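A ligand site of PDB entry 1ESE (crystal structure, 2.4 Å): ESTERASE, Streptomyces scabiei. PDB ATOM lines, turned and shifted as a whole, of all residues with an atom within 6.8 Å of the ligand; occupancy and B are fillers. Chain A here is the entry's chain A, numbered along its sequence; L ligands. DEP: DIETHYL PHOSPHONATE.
O3 of the ligand lies within hydrogen-bond range of N of Ser 14, 3.2 Å away.
OG of Ser 14 is bonded to P of the ligand, 1.7 Å away.
The side-chain amide nitrogen (ND2) of Asn 106 lies within hydrogen-bond range of an oxygen (O3) of the ligand (3.0 Å).
O3 of the ligand is in hydrogen-bond range of N of Gly 66 (3.0 Å).
An oxygen (O1) of the ligand is in hydrogen-bond range of a ring nitrogen (NE2) of His 283, 3.1 Å away.
OG of Ser 14 sits at hydrogen-bond distance from NE2 of His 283, at 2.8 Å.
The backbone carbonyl oxygen of Ser 14 sits at hydrogen-bond distance from the backbone NH of Phe 19 (3.2 Å).
The backbone carbonyl oxygen (O) of Gly 66 lies close to the side-chain amide nitrogen (ND2) of Asn 106, at 3.3 Å.
The side-chain amide nitrogen (ND2) of Asn 106 sits at hydrogen-bond distance from the backbone carbonyl oxygen (O) of Ala 67 (2.8 Å).
O of Trp 280 sits at hydrogen-bond distance from ND1 of His 283 (2.8 Å).
The side-chain carboxylate of Asp 13 lies within hydrogen-bond range of the backbone NH of Tyr 15 (3.2 Å).
The backbone NH of Gly 105 lies within hydrogen-bond range of the side-chain hydroxyl of Tyr 186.
The backbone carbonyl oxygen (O) of Gly 105 is in hydrogen-bond range of the backbone NH (N) of Phe 110 (3.0 Å).
Asp 13 touches the ligand (OD2 to C3, 3.3 Å).
Tyr 15 touches the ligand (CE1 to O2, 3.8 Å).
Phe 19 touches the ligand.
Gly 65 touches the ligand.
CA of Gly 105 touches C4 of the ligand (3.4 Å).
Leu 127 touches the ligand (CD2 to C2, 3.8 Å).
Hydrophobic or aromatic side chains within 4 Å of the ligand: Tyr 15, Phe 19, Leu 127 and His 283.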
ATOM      1  N   GLY A  12      14.328  18.561  -7.466  1.00  0.00           N
ATOM      2  CA  GLY A  12      14.881  19.086  -6.219  1.00  0.00           C
ATOM      3  C   GLY A  12      15.928  18.281  -5.494  1.00  0.00           C
ATOM      4  O   GLY A  12      16.294  17.183  -5.934  1.00  0.00           O
ATOM      5  N   ASP A  13      16.386  18.851  -4.399  1.00  0.00           N
ATOM      6  CA  ASP A  13      17.438  18.251  -3.582  1.00  0.00           C
ATOM      7  C   ASP A  13      16.662  17.455  -2.550  1.00  0.00           C
ATOM      8  O   ASP A  13      15.512  17.074  -2.763  1.00  0.00           O
ATOM      9  CB  ASP A  13      18.412  19.284  -3.050  1.00  0.00           C
ATOM     10  CG  ASP A  13      17.816  20.441  -2.281  1.00  0.00           C
ATOM     11  OD1 ASP A  13      16.611  20.314  -1.945  1.00  0.00           O
ATOM     12  OD2 ASP A  13      18.653  21.398  -2.049  1.00  0.00           O
ATOM     13  N   SER A  14      17.275  17.224  -1.403  1.00  0.00           N
ATOM     14  CA  SER A  14      16.714  16.360  -0.358  1.00  0.00           C
ATOM     15  C   SER A  14      15.675  17.088   0.544  1.00  0.00           C
ATOM     16  O   SER A  14      14.953  16.459   1.416  1.00  0.00           O
ATOM     17  CB  SER A  14      17.672  15.715   0.607  1.00  0.00           C
ATOM     18  OG  SER A  14      18.543  16.581   1.290  1.00  0.00           O
ATOM     19  N   TYR A  15      15.422  18.389   0.277  1.00  0.00           N
ATOM     20  CA  TYR A  15      14.355  19.159   0.989  1.00  0.00           C
ATOM     21  C   TYR A  15      13.058  19.072   0.219  1.00  0.00           C
ATOM     22  O   TYR A  15      12.023  19.559   0.685  1.00  0.00           O
ATOM     23  CB  TYR A  15      14.805  20.574   1.324  1.00  0.00           C
ATOM     24  CG  TYR A  15      15.717  20.676   2.518  1.00  0.00           C
ATOM     25  CD1 TYR A  15      17.025  20.212   2.502  1.00  0.00           C
ATOM     26  CD2 TYR A  15      15.301  21.270   3.708  1.00  0.00           C
ATOM     27  CE1 TYR A  15      17.896  20.305   3.576  1.00  0.00           C
ATOM     28  CE2 TYR A  15      16.127  21.355   4.817  1.00  0.00           C
ATOM     29  CZ  TYR A  15      17.412  20.872   4.759  1.00  0.00           C
ATOM     30  OH  TYR A  15      18.265  21.007   5.842  1.00  0.00           O
ATOM     31  N   PHE A  19      14.479  13.633   2.827  1.00  0.00           N
ATOM     32  CA  PHE A  19      15.465  12.732   3.373  1.00  0.00           C
ATOM     33  C   PHE A  19      14.911  12.591   4.796  1.00  0.00           C
ATOM     34  O   PHE A  19      14.559  13.668   5.294  1.00  0.00           O
ATOM     35  CB  PHE A  19      16.826  13.368   3.489  1.00  0.00           C
ATOM     36  CG  PHE A  19      17.766  12.456   4.174  1.00  0.00           C
ATOM     37  CD1 PHE A  19      18.278  11.374   3.468  1.00  0.00           C
ATOM     38  CD2 PHE A  19      18.081  12.661   5.538  1.00  0.00           C
ATOM     39  CE1 PHE A  19      19.185  10.525   4.103  1.00  0.00           C
ATOM     40  CE2 PHE A  19      18.953  11.808   6.168  1.00  0.00           C
ATOM     41  CZ  PHE A  19      19.520  10.737   5.448  1.00  0.00           C
ATOM     42  N   CYS A  34      18.068   7.884  -3.613  1.00  0.00           N
ATOM     43  CA  CYS A  34      17.610   9.281  -3.647  1.00  0.00           C
ATOM     44  C   CYS A  34      17.057   9.619  -2.263  1.00  0.00           C
ATOM     45  O   CYS A  34      16.938  10.807  -1.911  1.00  0.00           O
ATOM     46  CB  CYS A  34      16.607   9.529  -4.797  1.00  0.00           C
ATOM     47  SG  CYS A  34      17.477   9.738  -6.374  1.00  0.00           S
ATOM     48  N   PHE A  35      16.635   8.614  -1.516  1.00  0.00           N
ATOM     49  CA  PHE A  35      16.053   8.677  -0.151  1.00  0.00           C
ATOM     50  C   PHE A  35      14.839   9.585  -0.294  1.00  0.00           C
ATOM     51  O   PHE A  35      14.644  10.495   0.506  1.00  0.00           O
ATOM     52  CB  PHE A  35      16.957   9.105   0.993  1.00  0.00           C
ATOM     53  CG  PHE A  35      18.085   8.141   1.309  1.00  0.00           C
ATOM     54  CD1 PHE A  35      17.771   6.840   1.681  1.00  0.00           C
ATOM     55  CD2 PHE A  35      19.410   8.532   1.210  1.00  0.00           C
ATOM     56  CE1 PHE A  35      18.805   5.948   1.995  1.00  0.00           C
ATOM     57  CE2 PHE A  35      20.452   7.681   1.517  1.00  0.00           C
ATOM     58  CZ  PHE A  35      20.134   6.384   1.908  1.00  0.00           C
ATOM     59  N   CYS A  64      15.959  14.140  -5.521  1.00  0.00           N
ATOM     60  CA  CYS A  64      16.921  13.209  -5.087  1.00  0.00           C
ATOM     61  C   CYS A  64      17.885  13.895  -4.152  1.00  0.00           C
ATOM     62  O   CYS A  64      18.280  14.976  -4.587  1.00  0.00           O
ATOM     63  CB  CYS A  64      17.692  12.745  -6.333  1.00  0.00           C
ATOM     64  SG  CYS A  64      18.721  11.282  -6.045  1.00  0.00           S
ATOM     65  N   GLY A  65      18.160  13.168  -3.066  1.00  0.00           N
ATOM     66  CA  GLY A  65      19.112  13.772  -2.157  1.00  0.00           C
ATOM     67  C   GLY A  65      20.490  13.716  -2.869  1.00  0.00           C
ATOM     68  O   GLY A  65      20.934  12.792  -3.611  1.00  0.00           O
ATOM     69  N   GLY A  66      21.195  14.760  -2.472  1.00  0.00           N
ATOM     70  CA  GLY A  66      22.547  15.141  -2.844  1.00  0.00           C
ATOM     71  C   GLY A  66      22.599  16.020  -4.089  1.00  0.00           C
ATOM     72  O   GLY A  66      23.673  16.581  -4.311  1.00  0.00           O
ATOM     73  N   ALA A  67      21.524  16.153  -4.853  1.00  0.00           N
ATOM     74  CA  ALA A  67      21.422  16.886  -6.074  1.00  0.00           C
ATOM     75  C   ALA A  67      21.855  18.332  -5.988  1.00  0.00           C
ATOM     76  O   ALA A  67      21.316  19.098  -5.158  1.00  0.00           O
ATOM     77  CB  ALA A  67      19.959  16.758  -6.492  1.00  0.00           C
ATOM     78  N   GLY A 104      19.877  24.171  -4.785  1.00  0.00           N
ATOM     79  CA  GLY A 104      20.726  25.337  -4.314  1.00  0.00           C
ATOM     80  C   GLY A 104      21.556  25.098  -3.063  1.00  0.00           C
ATOM     81  O   GLY A 104      22.759  25.480  -2.996  1.00  0.00           O
ATOM     82  N   GLY A 105      20.966  24.472  -2.054  1.00  0.00           N
ATOM     83  CA  GLY A 105      21.718  24.173  -0.846  1.00  0.00           C
ATOM     84  C   GLY A 105      23.012  23.421  -1.136  1.00  0.00           C
ATOM     85  O   GLY A 105      24.089  23.858  -0.678  1.00  0.00           O
ATOM     86  N   ASN A 106      22.991  22.330  -1.876  1.00  0.00           N
ATOM     87  CA  ASN A 106      24.191  21.555  -2.220  1.00  0.00           C
ATOM     88  C   ASN A 106      25.189  22.351  -3.056  1.00  0.00           C
ATOM     89  O   ASN A 106      26.405  22.186  -2.986  1.00  0.00           O
ATOM     90  CB  ASN A 106      23.835  20.245  -2.975  1.00  0.00           C
ATOM     91  CG  ASN A 106      22.980  19.472  -2.004  1.00  0.00           C
ATOM     92  OD1 ASN A 106      23.322  19.697  -0.826  1.00  0.00           O
ATOM     93  ND2 ASN A 106      21.990  18.722  -2.432  1.00  0.00           N
ATOM     94  N   THR A 107      24.696  23.240  -3.915  1.00  0.00           N
ATOM     95  CA  THR A 107      25.690  23.957  -4.714  1.00  0.00           C
ATOM     96  C   THR A 107      26.354  24.923  -3.778  1.00  0.00           C
ATOM     97  O   THR A 107      27.535  25.126  -3.957  1.00  0.00           O
ATOM     98  CB  THR A 107      25.046  24.548  -6.025  1.00  0.00           C
ATOM     99  OG1 THR A 107      24.554  23.383  -6.784  1.00  0.00           O
ATOM    100  CG2 THR A 107      26.108  25.436  -6.703  1.00  0.00           C
ATOM    101  N   GLY A 109      26.805  24.353  -0.793  1.00  0.00           N
ATOM    102  CA  GLY A 109      27.493  23.310  -0.054  1.00  0.00           C
ATOM    103  C   GLY A 109      27.184  23.405   1.448  1.00  0.00           C
ATOM    104  O   GLY A 109      28.071  23.334   2.352  1.00  0.00           O
ATOM    105  N   PHE A 110      25.907  23.572   1.739  1.00  0.00           N
ATOM    106  CA  PHE A 110      25.500  23.718   3.150  1.00  0.00           C
ATOM    107  C   PHE A 110      25.955  22.468   3.911  1.00  0.00           C
ATOM    108  O   PHE A 110      26.293  22.714   5.084  1.00  0.00           O
ATOM    109  CB  PHE A 110      24.036  24.103   3.278  1.00  0.00           C
ATOM    110  CG  PHE A 110      23.774  24.771   4.606  1.00  0.00           C
ATOM    111  CD1 PHE A 110      23.932  26.143   4.813  1.00  0.00           C
ATOM    112  CD2 PHE A 110      23.379  23.936   5.674  1.00  0.00           C
ATOM    113  CE1 PHE A 110      23.706  26.683   6.070  1.00  0.00           C
ATOM    114  CE2 PHE A 110      23.139  24.476   6.960  1.00  0.00           C
ATOM    115  CZ  PHE A 110      23.309  25.866   7.156  1.00  0.00           C
ATOM    116  N   ASN A 111      26.032  21.292   3.352  1.00  0.00           N
ATOM    117  CA  ASN A 111      26.488  19.999   3.874  1.00  0.00           C
ATOM    118  C   ASN A 111      27.953  20.123   4.313  1.00  0.00           C
ATOM    119  O   ASN A 111      28.210  19.734   5.438  1.00  0.00           O
ATOM    120  CB  ASN A 111      26.406  18.746   2.949  1.00  0.00           C
ATOM    121  CG  ASN A 111      26.881  19.157   1.538  1.00  0.00           C
ATOM    122  OD1 ASN A 111      26.347  20.126   0.925  1.00  0.00           O
ATOM    123  ND2 ASN A 111      27.883  18.568   0.890  1.00  0.00           N
ATOM    124  N   LEU A 126      26.342   9.330   5.996  1.00  0.00           N
ATOM    125  CA  LEU A 126      25.569   9.294   4.762  1.00  0.00           C
ATOM    126  C   LEU A 126      25.162  10.671   4.263  1.00  0.00           C
ATOM    127  O   LEU A 126      24.177  10.867   3.522  1.00  0.00           O
ATOM    128  CB  LEU A 126      24.378   8.370   5.164  1.00  0.00           C
ATOM    129  CG  LEU A 126      24.616   6.877   5.324  1.00  0.00           C
ATOM    130  CD1 LEU A 126      23.614   6.233   6.273  1.00  0.00           C
ATOM    131  CD2 LEU A 126      24.523   6.267   3.920  1.00  0.00           C
ATOM    132  N   LEU A 127      25.868  11.681   4.668  1.00  0.00           N
ATOM    133  CA  LEU A 127      25.666  13.098   4.364  1.00  0.00           C
ATOM    134  C   LEU A 127      26.894  13.376   3.482  1.00  0.00           C
ATOM    135  O   LEU A 127      28.004  13.206   3.991  1.00  0.00           O
ATOM    136  CB  LEU A 127      25.523  13.857   5.663  1.00  0.00           C
ATOM    137  CG  LEU A 127      24.538  14.945   5.991  1.00  0.00           C
ATOM    138  CD1 LEU A 127      25.299  16.194   6.480  1.00  0.00           C
ATOM    139  CD2 LEU A 127      23.673  15.294   4.794  1.00  0.00           C
ATOM    140  N   PRO A 128      26.603  13.730   2.254  1.00  0.00           N
ATOM    141  CA  PRO A 128      27.617  14.013   1.248  1.00  0.00           C
ATOM    142  C   PRO A 128      28.445  15.281   1.497  1.00  0.00           C
ATOM    143  O   PRO A 128      27.981  16.270   2.097  1.00  0.00           O
ATOM    144  CB  PRO A 128      26.818  14.180  -0.054  1.00  0.00           C
ATOM    145  CG  PRO A 128      25.470  14.699   0.431  1.00  0.00           C
ATOM    146  CD  PRO A 128      25.232  13.899   1.708  1.00  0.00           C
ATOM    147  N   TYR A 186      14.233  26.840   1.573  1.00  0.00           N
ATOM    148  CA  TYR A 186      14.632  25.967   2.681  1.00  0.00           C
ATOM    149  C   TYR A 186      14.051  26.594   3.948  1.00  0.00           C
ATOM    150  O   TYR A 186      14.070  27.838   4.084  1.00  0.00           O
ATOM    151  CB  TYR A 186      16.155  25.827   2.792  1.00  0.00           C
ATOM    152  CG  TYR A 186      16.764  25.297   1.520  1.00  0.00           C
ATOM    153  CD1 TYR A 186      16.561  23.971   1.170  1.00  0.00           C
ATOM    154  CD2 TYR A 186      17.403  26.120   0.602  1.00  0.00           C
ATOM    155  CE1 TYR A 186      17.053  23.442  -0.031  1.00  0.00           C
ATOM    156  CE2 TYR A 186      17.913  25.618  -0.600  1.00  0.00           C
ATOM    157  CZ  TYR A 186      17.721  24.277  -0.904  1.00  0.00           C
ATOM    158  OH  TYR A 186      18.219  23.722  -2.046  1.00  0.00           O
ATOM    159  N   LEU A 227      21.545  32.767   1.240  1.00  0.00           N
ATOM    160  CA  LEU A 227      21.143  31.702   0.394  1.00  0.00           C
ATOM    161  C   LEU A 227      19.652  32.037   0.061  1.00  0.00           C
ATOM    162  O   LEU A 227      19.357  31.966  -1.110  1.00  0.00           O
ATOM    163  CB  LEU A 227      21.152  30.269   0.956  1.00  0.00           C
ATOM    164  CG  LEU A 227      20.670  29.282  -0.129  1.00  0.00           C
ATOM    165  CD1 LEU A 227      21.575  29.402  -1.369  1.00  0.00           C
ATOM    166  CD2 LEU A 227      20.667  27.834   0.341  1.00  0.00           C
ATOM    167  N   TRP A 280      18.582  12.358  11.165  1.00  0.00           N
ATOM    168  CA  TRP A 280      17.901  13.362  10.372  1.00  0.00           C
ATOM    169  C   TRP A 280      18.895  14.178   9.562  1.00  0.00           C
ATOM    170  O   TRP A 280      18.592  14.463   8.419  1.00  0.00           O
ATOM    171  CB  TRP A 280      17.085  14.327  11.214  1.00  0.00           C
ATOM    172  CG  TRP A 280      15.770  13.814  11.610  1.00  0.00           C
ATOM    173  CD1 TRP A 280      15.410  13.471  12.894  1.00  0.00           C
ATOM    174  CD2 TRP A 280      14.640  13.491  10.807  1.00  0.00           C
ATOM    175  NE1 TRP A 280      14.129  13.023  12.919  1.00  0.00           N
ATOM    176  CE2 TRP A 280      13.627  12.996  11.650  1.00  0.00           C
ATOM    177  CE3 TRP A 280      14.374  13.601   9.458  1.00  0.00           C
ATOM    178  CZ2 TRP A 280      12.363  12.638  11.224  1.00  0.00           C
ATOM    179  CZ3 TRP A 280      13.112  13.209   9.009  1.00  0.00           C
ATOM    180  CH2 TRP A 280      12.117  12.741   9.849  1.00  0.00           C
ATOM    181  N   TYR A 281      19.973  14.541  10.213  1.00  0.00           N
ATOM    182  CA  TYR A 281      21.035  15.344   9.595  1.00  0.00           C
ATOM    183  C   TYR A 281      20.443  16.745   9.265  1.00  0.00           C
ATOM    184  O   TYR A 281      20.805  17.407   8.257  1.00  0.00           O
ATOM    185  CB  TYR A 281      21.669  14.764   8.348  1.00  0.00           C
ATOM    186  CG  TYR A 281      22.356  13.432   8.297  1.00  0.00           C
ATOM    187  CD1 TYR A 281      23.454  13.267   9.146  1.00  0.00           C
ATOM    188  CD2 TYR A 281      21.955  12.398   7.424  1.00  0.00           C
ATOM    189  CE1 TYR A 281      24.164  12.084   9.140  1.00  0.00           C
ATOM    190  CE2 TYR A 281      22.675  11.203   7.433  1.00  0.00           C
ATOM    191  CZ  TYR A 281      23.776  11.067   8.286  1.00  0.00           C
ATOM    192  OH  TYR A 281      24.537   9.930   8.374  1.00  0.00           O
ATOM    193  N   HIS A 283      17.226  17.731   8.448  1.00  0.00           N
ATOM    194  CA  HIS A 283      16.265  17.774   7.328  1.00  0.00           C
ATOM    195  C   HIS A 283      14.880  17.841   7.975  1.00  0.00           C
ATOM    196  O   HIS A 283      14.817  17.408   9.144  1.00  0.00           O
ATOM    197  CB  HIS A 283      16.443  16.503   6.611  1.00  0.00           C
ATOM    198  CG  HIS A 283      17.679  16.406   5.788  1.00  0.00           C
ATOM    199  ND1 HIS A 283      18.960  16.114   6.177  1.00  0.00           N
ATOM    200  CD2 HIS A 283      17.735  16.605   4.449  1.00  0.00           C
ATOM    201  CE1 HIS A 283      19.756  16.139   5.124  1.00  0.00           C
ATOM    202  NE2 HIS A 283      19.036  16.426   4.070  1.00  0.00           N
HETATM  203  C1  DEP L   1      20.393  14.195   1.331  1.00  0.00           C
HETATM  204  C2  DEP L   1      21.248  13.449   2.454  1.00  0.00           C
HETATM  205  C3  DEP L   1      20.236  19.902   0.383  1.00  0.00           C
HETATM  206  C4  DEP L   1      20.804  21.358   0.803  1.00  0.00           C
HETATM  207  O1  DEP L   1      20.348  15.642   1.371  1.00  0.00           O
HETATM  208  O2  DEP L   1      20.306  18.645   1.210  1.00  0.00           O
HETATM  209  O3  DEP L   1      20.343  17.014  -0.610  1.00  0.00           O
HETATM  210  P   DEP L   1      20.005  17.107   0.648  1.00  0.00           P
